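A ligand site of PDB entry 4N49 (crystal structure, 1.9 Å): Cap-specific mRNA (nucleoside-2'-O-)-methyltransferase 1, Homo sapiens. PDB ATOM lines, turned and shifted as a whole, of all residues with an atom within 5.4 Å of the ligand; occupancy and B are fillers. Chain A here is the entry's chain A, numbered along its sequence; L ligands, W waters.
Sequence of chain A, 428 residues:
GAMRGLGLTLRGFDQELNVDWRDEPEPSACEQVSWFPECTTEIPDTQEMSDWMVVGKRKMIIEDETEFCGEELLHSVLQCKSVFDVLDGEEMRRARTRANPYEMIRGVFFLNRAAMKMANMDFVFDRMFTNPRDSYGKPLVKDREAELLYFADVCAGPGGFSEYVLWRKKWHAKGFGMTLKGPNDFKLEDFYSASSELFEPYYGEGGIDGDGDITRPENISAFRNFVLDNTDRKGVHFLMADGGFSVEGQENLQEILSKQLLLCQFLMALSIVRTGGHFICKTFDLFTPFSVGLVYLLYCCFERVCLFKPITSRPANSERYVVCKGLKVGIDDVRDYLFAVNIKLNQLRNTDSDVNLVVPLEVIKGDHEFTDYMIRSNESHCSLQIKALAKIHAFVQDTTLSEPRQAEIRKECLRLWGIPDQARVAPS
O of Asn 184 is in hydrogen-bond range of O4 of the ligand, at 3.3 Å. The side-chain hydroxyl of Thr 179 sits at hydrogen-bond distance from an oxygen (O4) of the ligand, 3.4 Å away. An oxygen (O4) of the ligand is in hydrogen-bond range of the backbone carbonyl oxygen (O) of Gly 157 (2.7 Å). An oxygen (O1) of the ligand lies within hydrogen-bond range of the backbone NH (N) of Phe 161 (3.0 Å). N of Gly 160 sits at hydrogen-bond distance from O2 of the ligand (2.8 Å). ND2 of Asn 112 sits at hydrogen-bond distance from O2 of the ligand. N of Ile 214 lies within hydrogen-bond range of N5 of the ligand (3.0 Å). N4 of the ligand sits at hydrogen-bond distance from OD1 of Asp 213 (2.9 Å). The backbone NH of Gly 159 lies within hydrogen-bond range of an oxygen (O2) of the ligand. An oxygen (O4) of the ligand lies within hydrogen-bond range of the backbone NH (N) of Gly 157 (3.3 Å). A nitrogen (N1) of the ligand lies within salt-bridge range of the side-chain carboxylate (OD2) of Asp 242 (2.8 Å). N6 of the ligand sits close to SG of Cys 155 (3.8 Å). N of Leu 180 is in hydrogen-bond range of N6 of the ligand (3.4 Å).
Water W3 lies within hydrogen-bond range of O of Leu 180 (2.7 Å), OG1 of Thr 179 (2.7 Å), O of Asn 184 (2.8 Å) and O5 of the ligand (2.8 Å). Water W9 bridges an oxygen (O5) of the ligand (2.9 Å) and the side-chain amide nitrogen (ND2) of Asn 184 (3.0 Å). Water W5 bridges the side-chain carboxylate of Asp 153 (2.6 Å) and a nitrogen (N1) of the ligand (3.0 Å). Water W6 lies within hydrogen-bond range of OD2 of Asp 153 (2.7 Å), O of Ala 156 (2.8 Å), N of Phe 161 (3.0 Å), N1 of the ligand (3.3 Å) and N of Gly 160 (3.5 Å).
N of Cys 155 lies within hydrogen-bond range of O of Met 178, at 3.0 Å. The side-chain carboxylate (OD1) of Asp 242 is in salt-bridge range of the side-chain amino group (NZ) of Lys 282 (2.9 Å). The side-chain carboxylate (OD1) of Asp 213 lies within hydrogen-bond range of the side-chain hydroxyl (OG1) of Thr 215, at 2.7 Å. N of Ala 156 is in hydrogen-bond range of OG1 of Thr 179 (3.2 Å). The backbone NH of Ala 114 lies close to the side-chain amide oxygen of Asn 112 (3.4 Å). The side-chain amide oxygen of Asn 112 is in hydrogen-bond range of the backbone NH of Ala 115 (3.1 Å). The backbone NH (N) of Gly 157 lies within hydrogen-bond range of the side-chain hydroxyl (OG1) of Thr 179 (3.0 Å).
O of Gly 212 sits close to N5 of the ligand (3.4 Å). Ala 114 touches the ligand. Ala 156 touches the ligand. Pro 158 touches the ligand (CD to O2, 3.4 Å). Thr 215 touches the ligand (CG2 to N4, 3.8 Å). Gly 244 touches the ligand (O to C11, 3.4 Å). Leu 261 touches the ligand. Hydrophobic or aromatic side chains within 4 Å of the ligand: Ala 114, Pro 158, Phe 161, Leu 180, Ile 214 and Leu 261. Of the 26 residues printed, 19 come within 4 Å of the ligand. Along chain A the residues within 4 Å of the ligand span positions 112 to 261.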
ATOM      1  N   LEU A 111     -29.406 -23.349 -25.382  1.00  0.00           N
ATOM      2  CA  LEU A 111     -27.978 -23.519 -25.519  1.00  0.00           C
ATOM      3  C   LEU A 111     -27.176 -23.090 -24.269  1.00  0.00           C
ATOM      4  O   LEU A 111     -26.058 -23.565 -24.050  1.00  0.00           O
ATOM      5  CB  LEU A 111     -27.477 -22.863 -26.832  1.00  0.00           C
ATOM      6  CG  LEU A 111     -27.456 -21.336 -27.017  1.00  0.00           C
ATOM      7  CD1 LEU A 111     -26.243 -20.713 -26.323  1.00  0.00           C
ATOM      8  CD2 LEU A 111     -27.463 -20.942 -28.481  1.00  0.00           C
ATOM      9  N   ASN A 112     -27.710 -22.206 -23.450  1.00  0.00           N
ATOM     10  CA  ASN A 112     -27.004 -21.834 -22.201  1.00  0.00           C
ATOM     11  C   ASN A 112     -27.983 -21.377 -21.127  1.00  0.00           C
ATOM     12  O   ASN A 112     -29.179 -21.193 -21.410  1.00  0.00           O
ATOM     13  CB  ASN A 112     -25.924 -20.769 -22.457  1.00  0.00           C
ATOM     14  CG  ASN A 112     -26.478 -19.495 -23.085  1.00  0.00           C
ATOM     15  OD1 ASN A 112     -27.697 -19.316 -23.148  1.00  0.00           O
ATOM     16  ND2 ASN A 112     -25.597 -18.596 -23.558  1.00  0.00           N
ATOM     17  N   ALA A 114     -28.041 -18.459 -19.877  1.00  0.00           N
ATOM     18  CA  ALA A 114     -28.409 -17.065 -20.168  1.00  0.00           C
ATOM     19  C   ALA A 114     -29.774 -17.011 -20.846  1.00  0.00           C
ATOM     20  O   ALA A 114     -30.563 -16.089 -20.619  1.00  0.00           O
ATOM     21  CB  ALA A 114     -27.346 -16.375 -21.047  1.00  0.00           C
ATOM     22  N   ALA A 115     -30.050 -17.997 -21.691  1.00  0.00           N
ATOM     23  CA  ALA A 115     -31.311 -18.056 -22.426  1.00  0.00           C
ATOM     24  C   ALA A 115     -32.515 -18.032 -21.457  1.00  0.00           C
ATOM     25  O   ALA A 115     -33.535 -17.384 -21.739  1.00  0.00           O
ATOM     26  CB  ALA A 115     -31.362 -19.322 -23.339  1.00  0.00           C
ATOM     27  N   ASP A 153     -30.160  -7.987 -30.908  1.00  0.00           N
ATOM     28  CA  ASP A 153     -29.444  -8.606 -29.762  1.00  0.00           C
ATOM     29  C   ASP A 153     -27.957  -8.235 -29.904  1.00  0.00           C
ATOM     30  O   ASP A 153     -27.321  -8.621 -30.882  1.00  0.00           O
ATOM     31  CB  ASP A 153     -29.587 -10.127 -29.871  1.00  0.00           C
ATOM     32  CG  ASP A 153     -29.322 -10.865 -28.579  1.00  0.00           C
ATOM     33  OD1 ASP A 153     -29.103 -10.216 -27.525  1.00  0.00           O
ATOM     34  OD2 ASP A 153     -29.330 -12.136 -28.631  1.00  0.00           O
ATOM     35  N   CYS A 155     -23.935  -7.673 -27.971  1.00  0.00           N
ATOM     36  CA  CYS A 155     -23.096  -8.173 -26.882  1.00  0.00           C
ATOM     37  C   CYS A 155     -23.720  -9.485 -26.416  1.00  0.00           C
ATOM     38  O   CYS A 155     -24.106  -9.634 -25.239  1.00  0.00           O
ATOM     39  CB  CYS A 155     -23.001  -7.159 -25.739  1.00  0.00           C
ATOM     40  SG  CYS A 155     -22.341  -5.530 -26.213  1.00  0.00           S
ATOM     41  N   ALA A 156     -23.811 -10.416 -27.353  1.00  0.00           N
ATOM     42  CA  ALA A 156     -24.875 -11.379 -27.413  1.00  0.00           C
ATOM     43  C   ALA A 156     -24.438 -12.814 -27.711  1.00  0.00           C
ATOM     44  O   ALA A 156     -25.255 -13.723 -27.664  1.00  0.00           O
ATOM     45  CB  ALA A 156     -25.851 -10.931 -28.482  1.00  0.00           C
ATOM     46  N   GLY A 157     -23.184 -13.008 -28.091  1.00  0.00           N
ATOM     47  CA  GLY A 157     -22.725 -14.367 -28.405  1.00  0.00           C
ATOM     48  C   GLY A 157     -22.631 -15.153 -27.110  1.00  0.00           C
ATOM     49  O   GLY A 157     -22.303 -14.577 -26.071  1.00  0.00           O
ATOM     50  N   PRO A 158     -22.909 -16.462 -27.140  1.00  0.00           N
ATOM     51  CA  PRO A 158     -23.250 -17.335 -28.268  1.00  0.00           C
ATOM     52  C   PRO A 158     -24.684 -17.207 -28.799  1.00  0.00           C
ATOM     53  O   PRO A 158     -24.950 -17.758 -29.865  1.00  0.00           O
ATOM     54  CB  PRO A 158     -23.022 -18.751 -27.701  1.00  0.00           C
ATOM     55  CG  PRO A 158     -23.312 -18.597 -26.251  1.00  0.00           C
ATOM     56  CD  PRO A 158     -22.732 -17.228 -25.908  1.00  0.00           C
ATOM     57  N   GLY A 159     -25.590 -16.545 -28.061  1.00  0.00           N
ATOM     58  CA  GLY A 159     -26.896 -16.256 -28.607  1.00  0.00           C
ATOM     59  C   GLY A 159     -28.135 -16.795 -27.903  1.00  0.00           C
ATOM     60  O   GLY A 159     -29.212 -16.805 -28.494  1.00  0.00           O
ATOM     61  N   GLY A 160     -28.009 -17.180 -26.638  1.00  0.00           N
ATOM     62  CA  GLY A 160     -29.162 -17.660 -25.885  1.00  0.00           C
ATOM     63  C   GLY A 160     -30.390 -16.760 -25.849  1.00  0.00           C
ATOM     64  O   GLY A 160     -31.527 -17.235 -25.923  1.00  0.00           O
ATOM     65  N   PHE A 161     -30.193 -15.462 -25.683  1.00  0.00           N
ATOM     66  CA  PHE A 161     -31.323 -14.553 -25.594  1.00  0.00           C
ATOM     67  C   PHE A 161     -32.111 -14.669 -26.898  1.00  0.00           C
ATOM     68  O   PHE A 161     -33.349 -14.682 -26.900  1.00  0.00           O
ATOM     69  CB  PHE A 161     -30.856 -13.082 -25.442  1.00  0.00           C
ATOM     70  CG  PHE A 161     -30.521 -12.665 -24.010  1.00  0.00           C
ATOM     71  CD1 PHE A 161     -30.293 -13.605 -23.030  1.00  0.00           C
ATOM     72  CD2 PHE A 161     -30.446 -11.314 -23.668  1.00  0.00           C
ATOM     73  CE1 PHE A 161     -29.993 -13.221 -21.729  1.00  0.00           C
ATOM     74  CE2 PHE A 161     -30.134 -10.935 -22.363  1.00  0.00           C
ATOM     75  CZ  PHE A 161     -29.940 -11.892 -21.391  1.00  0.00           C
ATOM     76  N   MET A 178     -25.212  -8.247 -33.109  1.00  0.00           N
ATOM     77  CA  MET A 178     -23.806  -7.843 -33.219  1.00  0.00           C
ATOM     78  C   MET A 178     -23.032  -8.197 -31.962  1.00  0.00           C
ATOM     79  O   MET A 178     -23.395  -7.744 -30.873  1.00  0.00           O
ATOM     80  CB  MET A 178     -23.639  -6.346 -33.484  1.00  0.00           C
ATOM     81  CG  MET A 178     -22.158  -5.955 -33.802  1.00  0.00           C
ATOM     82  SD  MET A 178     -21.969  -4.350 -34.628  1.00  0.00           S
ATOM     83  CE  MET A 178     -22.541  -3.240 -33.371  1.00  0.00           C
ATOM     84  N   THR A 179     -21.966  -8.968 -32.129  1.00  0.00           N
ATOM     85  CA  THR A 179     -21.143  -9.427 -31.013  1.00  0.00           C
ATOM     86  C   THR A 179     -19.687  -9.607 -31.512  1.00  0.00           C
ATOM     87  O   THR A 179     -19.457  -9.748 -32.719  1.00  0.00           O
ATOM     88  CB  THR A 179     -21.736 -10.720 -30.418  1.00  0.00           C
ATOM     89  OG1 THR A 179     -21.217 -10.955 -29.107  1.00  0.00           O
ATOM     90  CG2 THR A 179     -21.449 -11.912 -31.327  1.00  0.00           C
ATOM     91  N   LEU A 180     -18.720  -9.534 -30.618  1.00  0.00           N
ATOM     92  CA  LEU A 180     -17.306  -9.730 -30.994  1.00  0.00           C
ATOM     93  C   LEU A 180     -17.052 -11.084 -31.641  1.00  0.00           C
ATOM     94  O   LEU A 180     -17.684 -12.088 -31.275  1.00  0.00           O
ATOM     95  CB  LEU A 180     -16.409  -9.638 -29.767  1.00  0.00           C
ATOM     96  CG  LEU A 180     -16.313  -8.291 -29.092  1.00  0.00           C
ATOM     97  CD1 LEU A 180     -15.491  -8.422 -27.838  1.00  0.00           C
ATOM     98  CD2 LEU A 180     -15.690  -7.286 -30.045  1.00  0.00           C
ATOM     99  N   ASN A 184     -16.404 -16.409 -28.257  1.00  0.00           N
ATOM    100  CA  ASN A 184     -17.747 -16.123 -27.786  1.00  0.00           C
ATOM    101  C   ASN A 184     -18.668 -15.582 -28.854  1.00  0.00           C
ATOM    102  O   ASN A 184     -19.660 -14.926 -28.545  1.00  0.00           O
ATOM    103  CB  ASN A 184     -17.693 -15.149 -26.621  1.00  0.00           C
ATOM    104  CG  ASN A 184     -16.932 -15.710 -25.456  1.00  0.00           C
ATOM    105  OD1 ASN A 184     -17.192 -16.842 -25.034  1.00  0.00           O
ATOM    106  ND2 ASN A 184     -15.984 -14.944 -24.927  1.00  0.00           N
ATOM    107  N   GLY A 212     -17.133  -6.688 -34.994  1.00  0.00           N
ATOM    108  CA  GLY A 212     -18.320  -6.760 -34.143  1.00  0.00           C
ATOM    109  C   GLY A 212     -18.238  -5.944 -32.847  1.00  0.00           C
ATOM    110  O   GLY A 212     -19.064  -6.139 -31.953  1.00  0.00           O
ATOM    111  N   ASP A 213     -17.256  -5.038 -32.753  1.00  0.00           N
ATOM    112  CA  ASP A 213     -16.999  -4.270 -31.519  1.00  0.00           C
ATOM    113  C   ASP A 213     -17.972  -3.080 -31.389  1.00  0.00           C
ATOM    114  O   ASP A 213     -17.917  -2.112 -32.162  1.00  0.00           O
ATOM    115  CB  ASP A 213     -15.531  -3.790 -31.514  1.00  0.00           C
ATOM    116  CG  ASP A 213     -15.116  -3.138 -30.211  1.00  0.00           C
ATOM    117  OD1 ASP A 213     -15.981  -2.832 -29.356  1.00  0.00           O
ATOM    118  OD2 ASP A 213     -13.907  -2.886 -30.056  1.00  0.00           O
ATOM    119  N   ILE A 214     -18.862  -3.138 -30.410  1.00  0.00           N
ATOM    120  CA  ILE A 214     -19.911  -2.117 -30.274  1.00  0.00           C
ATOM    121  C   ILE A 214     -19.358  -0.786 -29.772  1.00  0.00           C
ATOM    122  O   ILE A 214     -20.068   0.227 -29.755  1.00  0.00           O
ATOM    123  CB  ILE A 214     -21.069  -2.622 -29.338  1.00  0.00           C
ATOM    124  CG1 ILE A 214     -22.367  -1.824 -29.583  1.00  0.00           C
ATOM    125  CG2 ILE A 214     -20.620  -2.595 -27.894  1.00  0.00           C
ATOM    126  CD1 ILE A 214     -23.539  -2.217 -28.682  1.00  0.00           C
ATOM    127  N   THR A 215     -18.080  -0.763 -29.402  1.00  0.00           N
ATOM    128  CA  THR A 215     -17.526   0.484 -28.868  1.00  0.00           C
ATOM    129  C   THR A 215     -16.873   1.366 -29.935  1.00  0.00           C
ATOM    130  O   THR A 215     -16.550   2.513 -29.677  1.00  0.00           O
ATOM    131  CB  THR A 215     -16.486   0.251 -27.748  1.00  0.00           C
ATOM    132  OG1 THR A 215     -15.321  -0.397 -28.294  1.00  0.00           O
ATOM    133  CG2 THR A 215     -17.067  -0.577 -26.614  1.00  0.00           C
ATOM    134  N   ASP A 242     -26.534  -7.696 -23.461  1.00  0.00           N
ATOM    135  CA  ASP A 242     -26.111  -8.546 -22.326  1.00  0.00           C
ATOM    136  C   ASP A 242     -24.583  -8.514 -22.126  1.00  0.00           C
ATOM    137  O   ASP A 242     -23.946  -9.530 -21.801  1.00  0.00           O
ATOM    138  CB  ASP A 242     -26.597  -9.976 -22.535  1.00  0.00           C
ATOM    139  CG  ASP A 242     -26.506 -10.821 -21.249  1.00  0.00           C
ATOM    140  OD1 ASP A 242     -26.649 -10.217 -20.154  1.00  0.00           O
ATOM    141  OD2 ASP A 242     -26.267 -12.054 -21.318  1.00  0.00           O
ATOM    142  N   GLY A 243     -24.015  -7.327 -22.305  1.00  0.00           N
ATOM    143  CA  GLY A 243     -22.560  -7.160 -22.349  1.00  0.00           C
ATOM    144  C   GLY A 243     -21.823  -7.460 -21.050  1.00  0.00           C
ATOM    145  O   GLY A 243     -22.219  -7.002 -19.978  1.00  0.00           O
ATOM    146  N   GLY A 244     -20.727  -8.221 -21.169  1.00  0.00           N
ATOM    147  CA  GLY A 244     -19.759  -8.383 -20.097  1.00  0.00           C
ATOM    148  C   GLY A 244     -18.469  -9.014 -20.626  1.00  0.00           C
ATOM    149  O   GLY A 244     -18.389  -9.412 -21.800  1.00  0.00           O
ATOM    150  N   PHE A 245     -17.463  -9.093 -19.762  1.00  0.00           N
ATOM    151  CA  PHE A 245     -16.204  -9.770 -20.092  1.00  0.00           C
ATOM    152  C   PHE A 245     -15.511 -10.100 -18.782  1.00  0.00           C
ATOM    153  O   PHE A 245     -15.913  -9.625 -17.722  1.00  0.00           O
ATOM    154  CB  PHE A 245     -15.299  -8.901 -20.979  1.00  0.00           C
ATOM    155  CG  PHE A 245     -15.140  -7.490 -20.475  1.00  0.00           C
ATOM    156  CD1 PHE A 245     -14.282  -7.203 -19.415  1.00  0.00           C
ATOM    157  CD2 PHE A 245     -15.860  -6.455 -21.044  1.00  0.00           C
ATOM    158  CE1 PHE A 245     -14.171  -5.909 -18.950  1.00  0.00           C
ATOM    159  CE2 PHE A 245     -15.740  -5.179 -20.577  1.00  0.00           C
ATOM    160  CZ  PHE A 245     -14.886  -4.897 -19.539  1.00  0.00           C
ATOM    161  N   LEU A 261     -18.710  -0.042 -22.288  1.00  0.00           N
ATOM    162  CA  LEU A 261     -19.646  -1.022 -22.790  1.00  0.00           C
ATOM    163  C   LEU A 261     -21.087  -0.669 -22.393  1.00  0.00           C
ATOM    164  O   LEU A 261     -22.009  -0.777 -23.204  1.00  0.00           O
ATOM    165  CB  LEU A 261     -19.272  -2.403 -22.241  1.00  0.00           C
ATOM    166  CG  LEU A 261     -19.786  -3.605 -23.013  1.00  0.00           C
ATOM    167  CD1 LEU A 261     -19.448  -3.438 -24.488  1.00  0.00           C
ATOM    168  CD2 LEU A 261     -19.158  -4.907 -22.450  1.00  0.00           C
ATOM    169  N   LYS A 282     -28.196  -5.772 -19.553  1.00  0.00           N
ATOM    170  CA  LYS A 282     -27.492  -6.108 -18.332  1.00  0.00           C
ATOM    171  C   LYS A 282     -26.635  -4.940 -17.800  1.00  0.00           C
ATOM    172  O   LYS A 282     -25.943  -4.259 -18.578  1.00  0.00           O
ATOM    173  CB  LYS A 282     -26.558  -7.340 -18.552  1.00  0.00           C
ATOM    174  CG  LYS A 282     -26.055  -7.964 -17.259  1.00  0.00           C
ATOM    175  CD  LYS A 282     -24.521  -8.213 -17.278  1.00  0.00           C
ATOM    176  CE  LYS A 282     -24.096  -9.240 -18.364  1.00  0.00           C
ATOM    177  NZ  LYS A 282     -24.592 -10.627 -18.104  1.00  0.00           N
HETATM  178  N1  LIG L   1     -26.970 -13.039 -23.828  1.00  0.00           N
HETATM  179  C1  LIG L   1     -25.972 -13.933 -24.449  1.00  0.00           C
HETATM  180  C2  LIG L   1     -26.506 -15.300 -24.588  1.00  0.00           C
HETATM  181  O1  LIG L   1     -27.657 -15.547 -24.125  1.00  0.00           O
HETATM  182  O2  LIG L   1     -25.870 -16.189 -25.126  1.00  0.00           O
HETATM  183  C3  LIG L   1     -24.752 -14.024 -23.598  1.00  0.00           C
HETATM  184  C4  LIG L   1     -23.863 -12.829 -23.695  1.00  0.00           C
HETATM  185  S1  LIG L   1     -22.280 -12.783 -22.785  1.00  0.00           S
HETATM  186  C5  LIG L   1     -22.567 -12.741 -21.087  1.00  0.00           C
HETATM  187  C6  LIG L   1     -21.460 -11.275 -23.241  1.00  0.00           C
HETATM  188  C7  LIG L   1     -21.220 -11.098 -24.707  1.00  0.00           C
HETATM  189  O3  LIG L   1     -20.906  -9.718 -24.957  1.00  0.00           O
HETATM  190  C8  LIG L   1     -20.080 -11.901 -25.144  1.00  0.00           C
HETATM  191  O4  LIG L   1     -20.433 -12.627 -26.298  1.00  0.00           O
HETATM  192  C9  LIG L   1     -19.026 -10.879 -25.385  1.00  0.00           C
HETATM  193  O5  LIG L   1     -18.085 -11.303 -26.314  1.00  0.00           O
HETATM  194  C10 LIG L   1     -19.798  -9.722 -25.845  1.00  0.00           C
HETATM  195  N2  LIG L   1     -19.068  -8.507 -25.885  1.00  0.00           N
HETATM  196  C11 LIG L   1     -18.224  -8.030 -24.944  1.00  0.00           C
HETATM  197  N3  LIG L   1     -17.684  -6.859 -25.324  1.00  0.00           N
HETATM  198  C12 LIG L   1     -18.211  -6.538 -26.535  1.00  0.00           C
HETATM  199  C13 LIG L   1     -18.018  -5.466 -27.453  1.00  0.00           C
HETATM  200  N4  LIG L   1     -17.121  -4.350 -27.137  1.00  0.00           N
HETATM  201  N5  LIG L   1     -18.688  -5.474 -28.609  1.00  0.00           N
HETATM  202  C14 LIG L   1     -19.563  -6.470 -28.933  1.00  0.00           C
HETATM  203  N6  LIG L   1     -19.735  -7.529 -28.093  1.00  0.00           N
HETATM  204  C15 LIG L   1     -19.081  -7.592 -26.908  1.00  0.00           C
HETATM  205  O   HOH W   1     -21.447 -14.873 -18.594  1.00  0.00           O
HETATM  206  O   HOH W   2     -23.726 -15.552 -19.763  1.00  0.00           O
HETATM  207  O   HOH W   3     -18.836 -12.240 -28.876  1.00  0.00           O
HETATM  208  O   HOH W   4     -22.576 -12.511 -17.689  1.00  0.00           O
HETATM  209  O   HOH W   5     -27.463 -10.669 -25.558  1.00  0.00           O
HETATM  210  O   HOH W   6     -27.984 -13.726 -26.865  1.00  0.00           O
HETATM  211  O   HOH W   7     -19.051 -13.745 -22.061  1.00  0.00           O
HETATM  212  O   HOH W   8     -15.585  -4.873 -24.792  1.00  0.00           O
HETATM  213  O   HOH W   9     -15.341 -12.247 -26.079  1.00  0.00           O
